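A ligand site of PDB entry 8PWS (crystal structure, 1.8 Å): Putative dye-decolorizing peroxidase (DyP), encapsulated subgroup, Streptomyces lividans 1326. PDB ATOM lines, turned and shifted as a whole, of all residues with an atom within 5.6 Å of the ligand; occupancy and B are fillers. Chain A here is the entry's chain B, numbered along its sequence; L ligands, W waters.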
ATOM      1  N   ASP A 140      23.247 -12.170 -22.990  1.00  0.00           N
ATOM      2  CA  ASP A 140      24.318 -12.424 -22.049  1.00  0.00           C
ATOM      3  C   ASP A 140      23.733 -12.800 -20.674  1.00  0.00           C
ATOM      4  O   ASP A 140      22.520 -12.964 -20.514  1.00  0.00           O
ATOM      5  CB  ASP A 140      25.298 -11.248 -22.030  1.00  0.00           C
ATOM      6  CG  ASP A 140      24.708  -9.946 -21.577  1.00  0.00           C
ATOM      7  OD1 ASP A 140      23.716  -9.982 -20.831  1.00  0.00           O
ATOM      8  OD2 ASP A 140      25.225  -8.899 -22.012  1.00  0.00           O
ATOM      9  N   LEU A 142      23.382 -11.129 -18.067  1.00  0.00           N
ATOM     10  CA  LEU A 142      22.534 -10.130 -17.477  1.00  0.00           C
ATOM     11  C   LEU A 142      21.156 -10.125 -18.167  1.00  0.00           C
ATOM     12  O   LEU A 142      20.281  -9.348 -17.782  1.00  0.00           O
ATOM     13  CB  LEU A 142      23.212  -8.767 -17.623  1.00  0.00           C
ATOM     14  CG  LEU A 142      24.562  -8.594 -16.928  1.00  0.00           C
ATOM     15  CD1 LEU A 142      25.059  -7.146 -17.072  1.00  0.00           C
ATOM     16  CD2 LEU A 142      24.486  -8.926 -15.460  1.00  0.00           C
ATOM     17  N   PHE A 144      20.476  -9.297 -21.381  1.00  0.00           N
ATOM     18  CA  PHE A 144      20.389  -8.332 -22.461  1.00  0.00           C
ATOM     19  C   PHE A 144      21.027  -8.888 -23.728  1.00  0.00           C
ATOM     20  O   PHE A 144      21.981  -9.661 -23.650  1.00  0.00           O
ATOM     21  CB  PHE A 144      21.074  -7.012 -22.086  1.00  0.00           C
ATOM     22  CG  PHE A 144      20.241  -6.136 -21.207  1.00  0.00           C
ATOM     23  CD1 PHE A 144      19.953  -6.481 -19.914  1.00  0.00           C
ATOM     24  CD2 PHE A 144      19.675  -4.997 -21.705  1.00  0.00           C
ATOM     25  CE1 PHE A 144      19.143  -5.696 -19.116  1.00  0.00           C
ATOM     26  CE2 PHE A 144      18.843  -4.190 -20.928  1.00  0.00           C
ATOM     27  CZ  PHE A 144      18.598  -4.523 -19.625  1.00  0.00           C
ATOM     28  N   VAL A 145      20.490  -8.503 -24.888  1.00  0.00           N
ATOM     29  CA  VAL A 145      21.091  -8.852 -26.157  1.00  0.00           C
ATOM     30  C   VAL A 145      22.467  -8.181 -26.203  1.00  0.00           C
ATOM     31  O   VAL A 145      22.626  -7.003 -25.816  1.00  0.00           O
ATOM     32  CB  VAL A 145      20.190  -8.421 -27.335  1.00  0.00           C
ATOM     33  CG1 VAL A 145      20.844  -8.789 -28.650  1.00  0.00           C
ATOM     34  CG2 VAL A 145      18.762  -8.995 -27.227  1.00  0.00           C
ATOM     35  N   ASP A 146      23.473  -8.924 -26.685  1.00  0.00           N
ATOM     36  CA  ASP A 146      24.857  -8.506 -26.546  1.00  0.00           C
ATOM     37  C   ASP A 146      25.543  -8.698 -27.902  1.00  0.00           C
ATOM     38  O   ASP A 146      25.602  -9.808 -28.389  1.00  0.00           O
ATOM     39  CB  ASP A 146      25.527  -9.320 -25.435  1.00  0.00           C
ATOM     40  CG  ASP A 146      26.882  -8.820 -24.951  1.00  0.00           C
ATOM     41  OD1 ASP A 146      27.677  -8.438 -25.830  1.00  0.00           O
ATOM     42  OD2 ASP A 146      27.172  -8.928 -23.688  1.00  0.00           O
ATOM     43  N   GLY A 147      25.961  -7.594 -28.532  1.00  0.00           N
ATOM     44  CA  GLY A 147      26.574  -7.610 -29.850  1.00  0.00           C
ATOM     45  C   GLY A 147      25.904  -6.704 -30.888  1.00  0.00           C
ATOM     46  O   GLY A 147      26.430  -6.479 -31.972  1.00  0.00           O
ATOM     47  N   THR A 148      24.759  -6.104 -30.523  1.00  0.00           N
ATOM     48  CA  THR A 148      23.858  -5.421 -31.438  1.00  0.00           C
ATOM     49  C   THR A 148      24.562  -4.350 -32.258  1.00  0.00           C
ATOM     50  O   THR A 148      24.406  -4.283 -33.451  1.00  0.00           O
ATOM     51  CB  THR A 148      22.729  -4.804 -30.627  1.00  0.00           C
ATOM     52  OG1 THR A 148      22.167  -5.847 -29.847  1.00  0.00           O
ATOM     53  CG2 THR A 148      21.667  -4.240 -31.537  1.00  0.00           C
ATOM     54  N   GLU A 149      25.352  -3.490 -31.602  1.00  0.00           N
ATOM     55  CA  GLU A 149      25.926  -2.361 -32.302  1.00  0.00           C
ATOM     56  C   GLU A 149      27.350  -2.656 -32.750  1.00  0.00           C
ATOM     57  O   GLU A 149      28.135  -1.736 -33.035  1.00  0.00           O
ATOM     58  CB  GLU A 149      25.924  -1.113 -31.423  1.00  0.00           C
ATOM     59  CG  GLU A 149      24.533  -0.500 -31.273  1.00  0.00           C
ATOM     60  CD  GLU A 149      23.894  -0.058 -32.578  1.00  0.00           C
ATOM     61  OE1 GLU A 149      24.455   0.760 -33.209  1.00  0.00           O
ATOM     62  OE2 GLU A 149      22.906  -0.576 -32.955  1.00  0.00           O
ATOM     63  N   ASN A 150      27.763  -3.932 -32.778  1.00  0.00           N
ATOM     64  CA  ASN A 150      29.046  -4.192 -33.395  1.00  0.00           C
ATOM     65  C   ASN A 150      29.010  -3.704 -34.834  1.00  0.00           C
ATOM     66  O   ASN A 150      28.013  -3.915 -35.505  1.00  0.00           O
ATOM     67  CB  ASN A 150      29.398  -5.670 -33.492  1.00  0.00           C
ATOM     68  CG  ASN A 150      30.116  -6.174 -32.268  1.00  0.00           C
ATOM     69  OD1 ASN A 150      30.907  -5.461 -31.653  1.00  0.00           O
ATOM     70  ND2 ASN A 150      29.842  -7.387 -31.884  1.00  0.00           N
ATOM     71  N   GLN A 178      39.031  -9.227 -20.636  1.00  0.00           N
ATOM     72  CA  GLN A 178      38.774  -9.135 -19.222  1.00  0.00           C
ATOM     73  C   GLN A 178      37.711 -10.201 -18.872  1.00  0.00           C
ATOM     74  O   GLN A 178      36.649 -10.275 -19.474  1.00  0.00           O
ATOM     75  CB  GLN A 178      38.173  -7.783 -18.850  1.00  0.00           C
ATOM     76  CG  GLN A 178      39.080  -6.616 -19.031  1.00  0.00           C
ATOM     77  CD  GLN A 178      38.370  -5.355 -18.630  1.00  0.00           C
ATOM     78  OE1 GLN A 178      37.378  -4.951 -19.224  1.00  0.00           O
ATOM     79  NE2 GLN A 178      38.845  -4.746 -17.573  1.00  0.00           N
ATOM     80  N   TYR A 180      34.901 -11.055 -16.346  1.00  0.00           N
ATOM     81  CA  TYR A 180      34.057 -10.409 -15.352  1.00  0.00           C
ATOM     82  C   TYR A 180      33.214 -11.466 -14.643  1.00  0.00           C
ATOM     83  O   TYR A 180      32.650 -12.342 -15.294  1.00  0.00           O
ATOM     84  CB  TYR A 180      33.102  -9.399 -15.991  1.00  0.00           C
ATOM     85  CG  TYR A 180      33.738  -8.084 -16.394  1.00  0.00           C
ATOM     86  CD1 TYR A 180      33.851  -7.035 -15.505  1.00  0.00           C
ATOM     87  CD2 TYR A 180      34.247  -7.894 -17.674  1.00  0.00           C
ATOM     88  CE1 TYR A 180      34.411  -5.830 -15.889  1.00  0.00           C
ATOM     89  CE2 TYR A 180      34.782  -6.679 -18.084  1.00  0.00           C
ATOM     90  CZ  TYR A 180      34.906  -5.658 -17.159  1.00  0.00           C
ATOM     91  OH  TYR A 180      35.501  -4.490 -17.543  1.00  0.00           O
ATOM     92  N   HIS A 182      29.741 -11.585 -12.137  1.00  0.00           N
ATOM     93  CA  HIS A 182      28.605 -10.744 -11.857  1.00  0.00           C
ATOM     94  C   HIS A 182      28.019 -11.075 -10.492  1.00  0.00           C
ATOM     95  O   HIS A 182      28.074 -12.204 -10.068  1.00  0.00           O
ATOM     96  CB  HIS A 182      27.511 -10.912 -12.907  1.00  0.00           C
ATOM     97  CG  HIS A 182      27.914 -10.450 -14.215  1.00  0.00           C
ATOM     98  ND1 HIS A 182      28.145  -9.133 -14.487  1.00  0.00           N
ATOM     99  CD2 HIS A 182      28.077 -11.131 -15.360  1.00  0.00           C
ATOM    100  CE1 HIS A 182      28.465  -9.032 -15.797  1.00  0.00           C
ATOM    101  NE2 HIS A 182      28.464 -10.252 -16.329  1.00  0.00           N
ATOM    102  N   ILE A 199      22.106  -0.238 -18.634  1.00  0.00           N
ATOM    103  CA  ILE A 199      22.687  -0.655 -19.904  1.00  0.00           C
ATOM    104  C   ILE A 199      22.532   0.479 -20.932  1.00  0.00           C
ATOM    105  O   ILE A 199      23.479   0.775 -21.640  1.00  0.00           O
ATOM    106  CB  ILE A 199      21.997  -1.945 -20.401  1.00  0.00           C
ATOM    107  CG1 ILE A 199      22.178  -3.111 -19.430  1.00  0.00           C
ATOM    108  CG2 ILE A 199      22.447  -2.309 -21.800  1.00  0.00           C
ATOM    109  CD1 ILE A 199      23.580  -3.496 -19.189  1.00  0.00           C
ATOM    110  N   ARG A 201      19.573   0.413 -23.072  1.00  0.00           N
ATOM    111  CA  ARG A 201      18.732  -0.141 -24.119  1.00  0.00           C
ATOM    112  C   ARG A 201      17.570  -0.846 -23.448  1.00  0.00           C
ATOM    113  O   ARG A 201      17.706  -1.263 -22.298  1.00  0.00           O
ATOM    114  CB  ARG A 201      19.475  -1.166 -24.990  1.00  0.00           C
ATOM    115  CG  ARG A 201      20.818  -0.679 -25.506  1.00  0.00           C
ATOM    116  CD  ARG A 201      21.463  -1.722 -26.404  1.00  0.00           C
ATOM    117  NE  ARG A 201      20.815  -1.930 -27.699  1.00  0.00           N
ATOM    118  CZ  ARG A 201      20.935  -1.150 -28.798  1.00  0.00           C
ATOM    119  NH1 ARG A 201      20.020  -1.210 -29.754  1.00  0.00           N
ATOM    120  NH2 ARG A 201      21.920  -0.269 -28.911  1.00  0.00           N
ATOM    121  N   ASP A 206      15.480  -4.577 -27.260  1.00  0.00           N
ATOM    122  CA  ASP A 206      16.832  -4.161 -27.588  1.00  0.00           C
ATOM    123  C   ASP A 206      16.839  -2.847 -28.390  1.00  0.00           C
ATOM    124  O   ASP A 206      17.764  -2.574 -29.123  1.00  0.00           O
ATOM    125  CB  ASP A 206      17.552  -5.209 -28.420  1.00  0.00           C
ATOM    126  CG  ASP A 206      19.063  -5.111 -28.450  1.00  0.00           C
ATOM    127  OD1 ASP A 206      19.668  -4.447 -27.562  1.00  0.00           O
ATOM    128  OD2 ASP A 206      19.634  -5.707 -29.340  1.00  0.00           O
ATOM    129  N   GLU A 208      17.491   1.073 -28.421  1.00  0.00           N
ATOM    130  CA  GLU A 208      18.240   2.038 -27.625  1.00  0.00           C
ATOM    131  C   GLU A 208      17.301   3.058 -26.952  1.00  0.00           C
ATOM    132  O   GLU A 208      16.351   3.472 -27.549  1.00  0.00           O
ATOM    133  CB  GLU A 208      19.276   2.638 -28.558  1.00  0.00           C
ATOM    134  CG  GLU A 208      20.208   3.607 -27.912  1.00  0.00           C
ATOM    135  CD  GLU A 208      21.360   4.008 -28.820  1.00  0.00           C
ATOM    136  OE1 GLU A 208      21.518   3.473 -29.902  1.00  0.00           O
ATOM    137  OE2 GLU A 208      22.137   4.800 -28.393  1.00  0.00           O
ATOM    138  N   HIS A 219      25.927   2.174 -19.666  1.00  0.00           N
ATOM    139  CA  HIS A 219      27.014   1.481 -20.342  1.00  0.00           C
ATOM    140  C   HIS A 219      27.143   1.976 -21.787  1.00  0.00           C
ATOM    141  O   HIS A 219      28.259   2.231 -22.258  1.00  0.00           O
ATOM    142  CB  HIS A 219      26.778  -0.034 -20.263  1.00  0.00           C
ATOM    143  CG  HIS A 219      27.807  -0.836 -20.893  1.00  0.00           C
ATOM    144  ND1 HIS A 219      29.111  -0.705 -20.518  1.00  0.00           N
ATOM    145  CD2 HIS A 219      27.762  -1.771 -21.858  1.00  0.00           C
ATOM    146  CE1 HIS A 219      29.855  -1.535 -21.252  1.00  0.00           C
ATOM    147  NE2 HIS A 219      29.055  -2.222 -22.059  1.00  0.00           N
ATOM    148  N   VAL A 220      26.005   2.121 -22.468  1.00  0.00           N
ATOM    149  CA  VAL A 220      26.020   2.556 -23.852  1.00  0.00           C
ATOM    150  C   VAL A 220      26.485   4.000 -23.944  1.00  0.00           C
ATOM    151  O   VAL A 220      27.208   4.321 -24.899  1.00  0.00           O
ATOM    152  CB  VAL A 220      24.652   2.330 -24.529  1.00  0.00           C
ATOM    153  CG1 VAL A 220      24.416   3.213 -25.748  1.00  0.00           C
ATOM    154  CG2 VAL A 220      24.499   0.851 -24.842  1.00  0.00           C
ATOM    155  N   THR A 223      30.428   3.982 -23.366  1.00  0.00           N
ATOM    156  CA  THR A 223      31.249   3.301 -24.363  1.00  0.00           C
ATOM    157  C   THR A 223      31.007   3.839 -25.768  1.00  0.00           C
ATOM    158  O   THR A 223      31.501   3.257 -26.710  1.00  0.00           O
ATOM    159  CB  THR A 223      31.040   1.778 -24.293  1.00  0.00           C
ATOM    160  OG1 THR A 223      29.668   1.443 -24.509  1.00  0.00           O
ATOM    161  CG2 THR A 223      31.525   1.220 -22.977  1.00  0.00           C
ATOM    162  N   SER A 224      30.223   4.915 -25.905  1.00  0.00           N
ATOM    163  CA  SER A 224      30.091   5.637 -27.174  1.00  0.00           C
ATOM    164  C   SER A 224      31.119   6.747 -27.183  1.00  0.00           C
ATOM    165  O   SER A 224      31.106   7.604 -26.315  1.00  0.00           O
ATOM    166  CB  SER A 224      28.711   6.205 -27.356  1.00  0.00           C
ATOM    167  OG  SER A 224      27.770   5.140 -27.448  1.00  0.00           O
ATOM    168  N   ILE A 235      34.672  -0.631 -31.800  1.00  0.00           N
ATOM    169  CA  ILE A 235      35.410  -1.854 -31.607  1.00  0.00           C
ATOM    170  C   ILE A 235      34.502  -3.021 -31.959  1.00  0.00           C
ATOM    171  O   ILE A 235      33.302  -2.866 -32.124  1.00  0.00           O
ATOM    172  CB  ILE A 235      35.934  -2.005 -30.175  1.00  0.00           C
ATOM    173  CG1 ILE A 235      34.818  -2.192 -29.148  1.00  0.00           C
ATOM    174  CG2 ILE A 235      36.833  -0.832 -29.802  1.00  0.00           C
ATOM    175  CD1 ILE A 235      35.387  -2.535 -27.793  1.00  0.00           C
ATOM    176  N   ARG A 237      33.319  -6.712 -30.601  1.00  0.00           N
ATOM    177  CA  ARG A 237      33.246  -7.476 -29.357  1.00  0.00           C
ATOM    178  C   ARG A 237      32.628  -8.837 -29.606  1.00  0.00           C
ATOM    179  O   ARG A 237      31.858  -8.978 -30.512  1.00  0.00           O
ATOM    180  CB  ARG A 237      32.385  -6.770 -28.302  1.00  0.00           C
ATOM    181  CG  ARG A 237      32.909  -5.421 -27.867  1.00  0.00           C
ATOM    182  CD  ARG A 237      31.831  -4.655 -27.118  1.00  0.00           C
ATOM    183  NE  ARG A 237      30.848  -4.173 -28.065  1.00  0.00           N
ATOM    184  CZ  ARG A 237      29.547  -4.477 -28.060  1.00  0.00           C
ATOM    185  NH1 ARG A 237      29.038  -5.182 -27.078  1.00  0.00           N
ATOM    186  NH2 ARG A 237      28.767  -4.081 -29.046  1.00  0.00           N
ATOM    187  N   ASN A 239      31.600 -11.026 -26.614  1.00  0.00           N
ATOM    188  CA  ASN A 239      31.466 -11.366 -25.205  1.00  0.00           C
ATOM    189  C   ASN A 239      30.711 -12.691 -25.063  1.00  0.00           C
ATOM    190  O   ASN A 239      29.736 -12.971 -25.781  1.00  0.00           O
ATOM    191  CB  ASN A 239      30.649 -10.292 -24.473  1.00  0.00           C
ATOM    192  CG  ASN A 239      31.264  -8.915 -24.545  1.00  0.00           C
ATOM    193  OD1 ASN A 239      32.464  -8.773 -24.866  1.00  0.00           O
ATOM    194  ND2 ASN A 239      30.439  -7.911 -24.312  1.00  0.00           N
ATOM    195  N   THR A 252      30.788 -12.880 -17.541  1.00  0.00           N
ATOM    196  CA  THR A 252      30.906 -12.457 -18.918  1.00  0.00           C
ATOM    197  C   THR A 252      32.388 -12.380 -19.236  1.00  0.00           C
ATOM    198  O   THR A 252      33.127 -11.705 -18.544  1.00  0.00           O
ATOM    199  CB  THR A 252      30.289 -11.079 -19.157  1.00  0.00           C
ATOM    200  OG1 THR A 252      28.892 -11.146 -18.889  1.00  0.00           O
ATOM    201  CG2 THR A 252      30.477 -10.586 -20.585  1.00  0.00           C
ATOM    202  N   PHE A 254      34.744 -10.767 -21.593  1.00  0.00           N
ATOM    203  CA  PHE A 254      34.831  -9.662 -22.531  1.00  0.00           C
ATOM    204  C   PHE A 254      36.041  -9.841 -23.431  1.00  0.00           C
ATOM    205  O   PHE A 254      37.137 -10.067 -22.941  1.00  0.00           O
ATOM    206  CB  PHE A 254      35.036  -8.330 -21.794  1.00  0.00           C
ATOM    207  CG  PHE A 254      35.303  -7.186 -22.727  1.00  0.00           C
ATOM    208  CD1 PHE A 254      34.282  -6.609 -23.485  1.00  0.00           C
ATOM    209  CD2 PHE A 254      36.597  -6.720 -22.897  1.00  0.00           C
ATOM    210  CE1 PHE A 254      34.543  -5.558 -24.340  1.00  0.00           C
ATOM    211  CE2 PHE A 254      36.859  -5.714 -23.807  1.00  0.00           C
ATOM    212  CZ  PHE A 254      35.827  -5.153 -24.527  1.00  0.00           C
ATOM    213  N   THR A 264      39.989   1.131 -27.354  1.00  0.00           N
ATOM    214  CA  THR A 264      39.521   0.291 -26.274  1.00  0.00           C
ATOM    215  C   THR A 264      39.898   0.888 -24.918  1.00  0.00           C
ATOM    216  O   THR A 264      39.092   0.885 -23.996  1.00  0.00           O
ATOM    217  CB  THR A 264      40.043  -1.144 -26.437  1.00  0.00           C
ATOM    218  OG1 THR A 264      39.798  -1.603 -27.748  1.00  0.00           O
ATOM    219  CG2 THR A 264      39.361  -2.112 -25.511  1.00  0.00           C
ATOM    220  N   MET A 267      37.671   3.756 -23.883  1.00  0.00           N
ATOM    221  CA  MET A 267      36.398   3.272 -23.380  1.00  0.00           C
ATOM    222  C   MET A 267      36.560   2.772 -21.943  1.00  0.00           C
ATOM    223  O   MET A 267      35.716   3.042 -21.076  1.00  0.00           O
ATOM    224  CB  MET A 267      35.900   2.133 -24.263  1.00  0.00           C
ATOM    225  CG  MET A 267      35.389   2.586 -25.585  1.00  0.00           C
ATOM    226  SD  MET A 267      35.015   1.180 -26.696  1.00  0.00           S
ATOM    227  CE  MET A 267      34.477   2.069 -28.149  1.00  0.00           C
ATOM    228  N   LEU A 268      37.642   2.025 -21.670  1.00  0.00           N
ATOM    229  CA  LEU A 268      37.893   1.537 -20.318  1.00  0.00           C
ATOM    230  C   LEU A 268      38.085   2.686 -19.320  1.00  0.00           C
ATOM    231  O   LEU A 268      37.625   2.587 -18.192  1.00  0.00           O
ATOM    232  CB  LEU A 268      39.109   0.630 -20.330  1.00  0.00           C
ATOM    233  CG  LEU A 268      38.839  -0.778 -20.860  1.00  0.00           C
ATOM    234  CD1 LEU A 268      40.134  -1.567 -21.041  1.00  0.00           C
ATOM    235  CD2 LEU A 268      37.925  -1.540 -19.949  1.00  0.00           C
ATOM    236  N   MET A 271      34.743   4.066 -18.468  1.00  0.00           N
ATOM    237  CA  MET A 271      34.003   3.147 -17.618  1.00  0.00           C
ATOM    238  C   MET A 271      34.503   3.165 -16.166  1.00  0.00           C
ATOM    239  O   MET A 271      33.695   3.195 -15.246  1.00  0.00           O
ATOM    240  CB  MET A 271      34.108   1.710 -18.154  1.00  0.00           C
ATOM    241  CG  MET A 271      33.301   1.476 -19.406  1.00  0.00           C
ATOM    242  SD  MET A 271      33.590  -0.214 -20.004  1.00  0.00           S
ATOM    243  CE  MET A 271      32.888  -1.220 -18.705  1.00  0.00           C
ATOM    244  N   ILE A 283      27.346  -0.512 -15.029  1.00  0.00           N
ATOM    245  CA  ILE A 283      27.444  -1.957 -15.158  1.00  0.00           C
ATOM    246  C   ILE A 283      28.490  -2.506 -14.177  1.00  0.00           C
ATOM    247  O   ILE A 283      28.400  -3.667 -13.768  1.00  0.00           O
ATOM    248  CB  ILE A 283      27.728  -2.353 -16.614  1.00  0.00           C
ATOM    249  CG1 ILE A 283      27.116  -3.712 -16.949  1.00  0.00           C
ATOM    250  CG2 ILE A 283      29.210  -2.276 -16.946  1.00  0.00           C
ATOM    251  CD1 ILE A 283      27.237  -4.048 -18.437  1.00  0.00           C
ATOM    252  N   LEU A 284      29.473  -1.685 -13.782  1.00  0.00           N
ATOM    253  CA  LEU A 284      30.528  -2.129 -12.872  1.00  0.00           C
ATOM    254  C   LEU A 284      30.004  -2.290 -11.451  1.00  0.00           C
ATOM    255  O   LEU A 284      30.650  -2.942 -10.660  1.00  0.00           O
ATOM    256  CB  LEU A 284      31.709  -1.164 -12.913  1.00  0.00           C
ATOM    257  CG  LEU A 284      32.426  -1.092 -14.251  1.00  0.00           C
ATOM    258  CD1 LEU A 284      33.488  -0.032 -14.267  1.00  0.00           C
ATOM    259  CD2 LEU A 284      33.016  -2.416 -14.659  1.00  0.00           C
ATOM    260  N   SER A 287      29.462  -6.000 -11.753  1.00  0.00           N
ATOM    261  CA  SER A 287      30.431  -6.735 -12.545  1.00  0.00           C
ATOM    262  C   SER A 287      31.829  -6.415 -12.018  1.00  0.00           C
ATOM    263  O   SER A 287      32.201  -5.245 -12.009  1.00  0.00           O
ATOM    264  CB  SER A 287      30.345  -6.353 -14.010  1.00  0.00           C
ATOM    265  OG  SER A 287      28.997  -6.328 -14.462  1.00  0.00           O
HETATM  266  C1  LIG L   1      27.391  -2.521 -25.692  1.00  0.00           C
HETATM  267  C2  LIG L   1      27.213  -5.858 -22.216  1.00  0.00           C
HETATM  268  C3  LIG L   1      31.828  -4.808 -20.978  1.00  0.00           C
HETATM  269  C4  LIG L   1      32.097  -1.904 -24.756  1.00  0.00           C
HETATM  270  C5  LIG L   1      27.010  -3.465 -24.755  1.00  0.00           C
HETATM  271  C6  LIG L   1      25.657  -3.886 -24.690  1.00  0.00           C
HETATM  272  C7  LIG L   1      25.608  -4.868 -23.769  1.00  0.00           C
HETATM  273  C8  LIG L   1      26.937  -4.993 -23.225  1.00  0.00           C
HETATM  274  C9  LIG L   1      24.416  -5.639 -23.327  1.00  0.00           C
HETATM  275  C10 LIG L   1      24.525  -3.390 -25.534  1.00  0.00           C
HETATM  276  C11 LIG L   1      24.271  -4.182 -26.846  1.00  0.00           C
HETATM  277  C12 LIG L   1      25.466  -4.110 -27.845  1.00  0.00           C
HETATM  278  O1  LIG L   1      26.359  -5.050 -27.745  1.00  0.00           O
HETATM  279  O2  LIG L   1      25.577  -3.162 -28.733  1.00  0.00           O
HETATM  280  C13 LIG L   1      28.451  -5.815 -21.625  1.00  0.00           C
HETATM  281  C14 LIG L   1      28.790  -6.612 -20.517  1.00  0.00           C
HETATM  282  C15 LIG L   1      30.055  -6.389 -20.138  1.00  0.00           C
HETATM  283  C16 LIG L   1      30.530  -5.327 -21.039  1.00  0.00           C
HETATM  284  C17 LIG L   1      27.873  -7.595 -19.835  1.00  0.00           C
HETATM  285  C18 LIG L   1      30.563  -7.026 -18.911  1.00  0.00           C
HETATM  286  C19 LIG L   1      31.170  -6.304 -18.026  1.00  0.00           C
HETATM  287  C20 LIG L   1      32.325  -3.917 -21.914  1.00  0.00           C
HETATM  288  C21 LIG L   1      33.627  -3.375 -21.932  1.00  0.00           C
HETATM  289  C22 LIG L   1      33.718  -2.530 -22.990  1.00  0.00           C
HETATM  290  C23 LIG L   1      32.412  -2.554 -23.599  1.00  0.00           C
HETATM  291  C24 LIG L   1      34.644  -3.770 -20.993  1.00  0.00           C
HETATM  292  C25 LIG L   1      34.855  -1.758 -23.564  1.00  0.00           C
HETATM  293  C26 LIG L   1      36.058  -1.588 -23.120  1.00  0.00           C
HETATM  294  C27 LIG L   1      30.842  -1.854 -25.351  1.00  0.00           C
HETATM  295  C28 LIG L   1      30.594  -1.056 -26.572  1.00  0.00           C
HETATM  296  C29 LIG L   1      29.286  -1.209 -26.789  1.00  0.00           C
HETATM  297  C30 LIG L   1      28.730  -2.108 -25.770  1.00  0.00           C
HETATM  298  C31 LIG L   1      31.499  -0.184 -27.396  1.00  0.00           C
HETATM  299  C32 LIG L   1      28.595  -0.487 -27.950  1.00  0.00           C
HETATM  300  C33 LIG L   1      28.018   0.890 -27.539  1.00  0.00           C
HETATM  301  C34 LIG L   1      27.303   1.611 -28.705  1.00  0.00           C
HETATM  302  O3  LIG L   1      26.091   1.411 -28.713  1.00  0.00           O
HETATM  303  O4  LIG L   1      27.836   2.353 -29.592  1.00  0.00           O
HETATM  304  N1  LIG L   1      27.788  -4.135 -23.874  1.00  0.00           N
HETATM  305  N2  LIG L   1      29.500  -5.038 -21.872  1.00  0.00           N
HETATM  306  N3  LIG L   1      31.586  -3.409 -22.931  1.00  0.00           N
HETATM  307  N4  LIG L   1      29.724  -2.495 -24.922  1.00  0.00           N
HETATM  308 FE1  LIG L   1      29.640  -3.701 -23.410  1.00  0.00          FE
HETATM  309  O   HOH W   1      24.568  -0.625 -27.844  1.00  0.00           O
HETATM  310  O   HOH W   2      30.638   2.598 -29.212  1.00  0.00           O
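The side-chain hydroxyl (OG1) of Thr 223 lies within hydrogen-bond range of the backbone carbonyl oxygen (O) of His 219, at 2.8 Å. The side-chain carboxylate of Asp 146 is in salt-bridge range of the guanidinium group of Arg 237 (3.7 Å). OG1 of Thr 148 sits at hydrogen-bond distance from OD2 of Asp 206 (2.6 Å). The backbone NH (N) of Phe 254 is in hydrogen-bond range of the backbone carbonyl oxygen (O) of Gln 178 (2.9 Å). The side-chain carboxylate (OD2) of Asp 146 sits close to the side-chain carboxylate (OD2) of Asp 140 (2.6 Å). The side-chain amide oxygen (OE1) of Gln 178 is in hydrogen-bond range of the side-chain hydroxyl (OH) of Tyr 180 (2.6 Å). The side-chain carboxylate (OD1) of Asp 140 is in hydrogen-bond range of the backbone NH (N) of Leu 142. OG1 of Thr 252 sits at hydrogen-bond distance from NE2 of His 182.
NE2 of His 219 is bound to FE1 of the ligand (2.1 Å). The backbone NH of Gly 147 sits at hydrogen-bond distance from an oxygen (O1) of the ligand, 2.7 Å away. NH1 of Arg 237 is in salt-bridge range of O1 of the ligand, at 2.8 Å. N of Glu 149 lies within hydrogen-bond range of O2 of the ligand (2.9 Å). N of Thr 148 is in hydrogen-bond range of O1 of the ligand (3.4 Å).
Water W1 bridges an oxygen (O3) of the ligand and the guanidinium group of Arg 201. Water W2 bridges the backbone carbonyl oxygen (O) of Thr 223 and an oxygen (O4) of the ligand.
Merely in contact with the ligand: Asp 140 (3.6 Å), Leu 142 (3.97 Å), Phe 144 (3.8 Å), Val 145 (3.4 Å), Asp 146 (3.4 Å), Gln 178 (3.5 Å), Tyr 180 (3.5 Å), Arg 201 (3.6 Å), Val 220 (3.9 Å), Thr 223 (3.4 Å), Ser 224 (3.5 Å), Asn 239 (3.9 Å), Thr 252 (3.8 Å), Phe 254 (3.4 Å), Met 267 (3.8 Å), Leu 268 (3.7 Å), Met 271 (3.7 Å) and Ile 283 (3.6 Å). Hydrophobic or aromatic side chains within 4 Å of the ligand: Leu 142, Phe 144, Tyr 180, His 219, Val 220, Phe 254, Met 267, Leu 268, Met 271 and Ile 283. 23 residues have an atom within 4 Å of the ligand: Asp 140, Leu 142, Phe 144, Val 145, Asp 146, Gly 147, Thr 148, Glu 149, Gln 178, Tyr 180, Arg 201, His 219, Val 220, Thr 223, Ser 224, Arg 237, Asn 239, Thr 252, Phe 254, Met 267, Leu 268, Met 271 and Ile 283. The nearest printed residue that does not touch the ligand is Thr 264 (4.01 Å).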
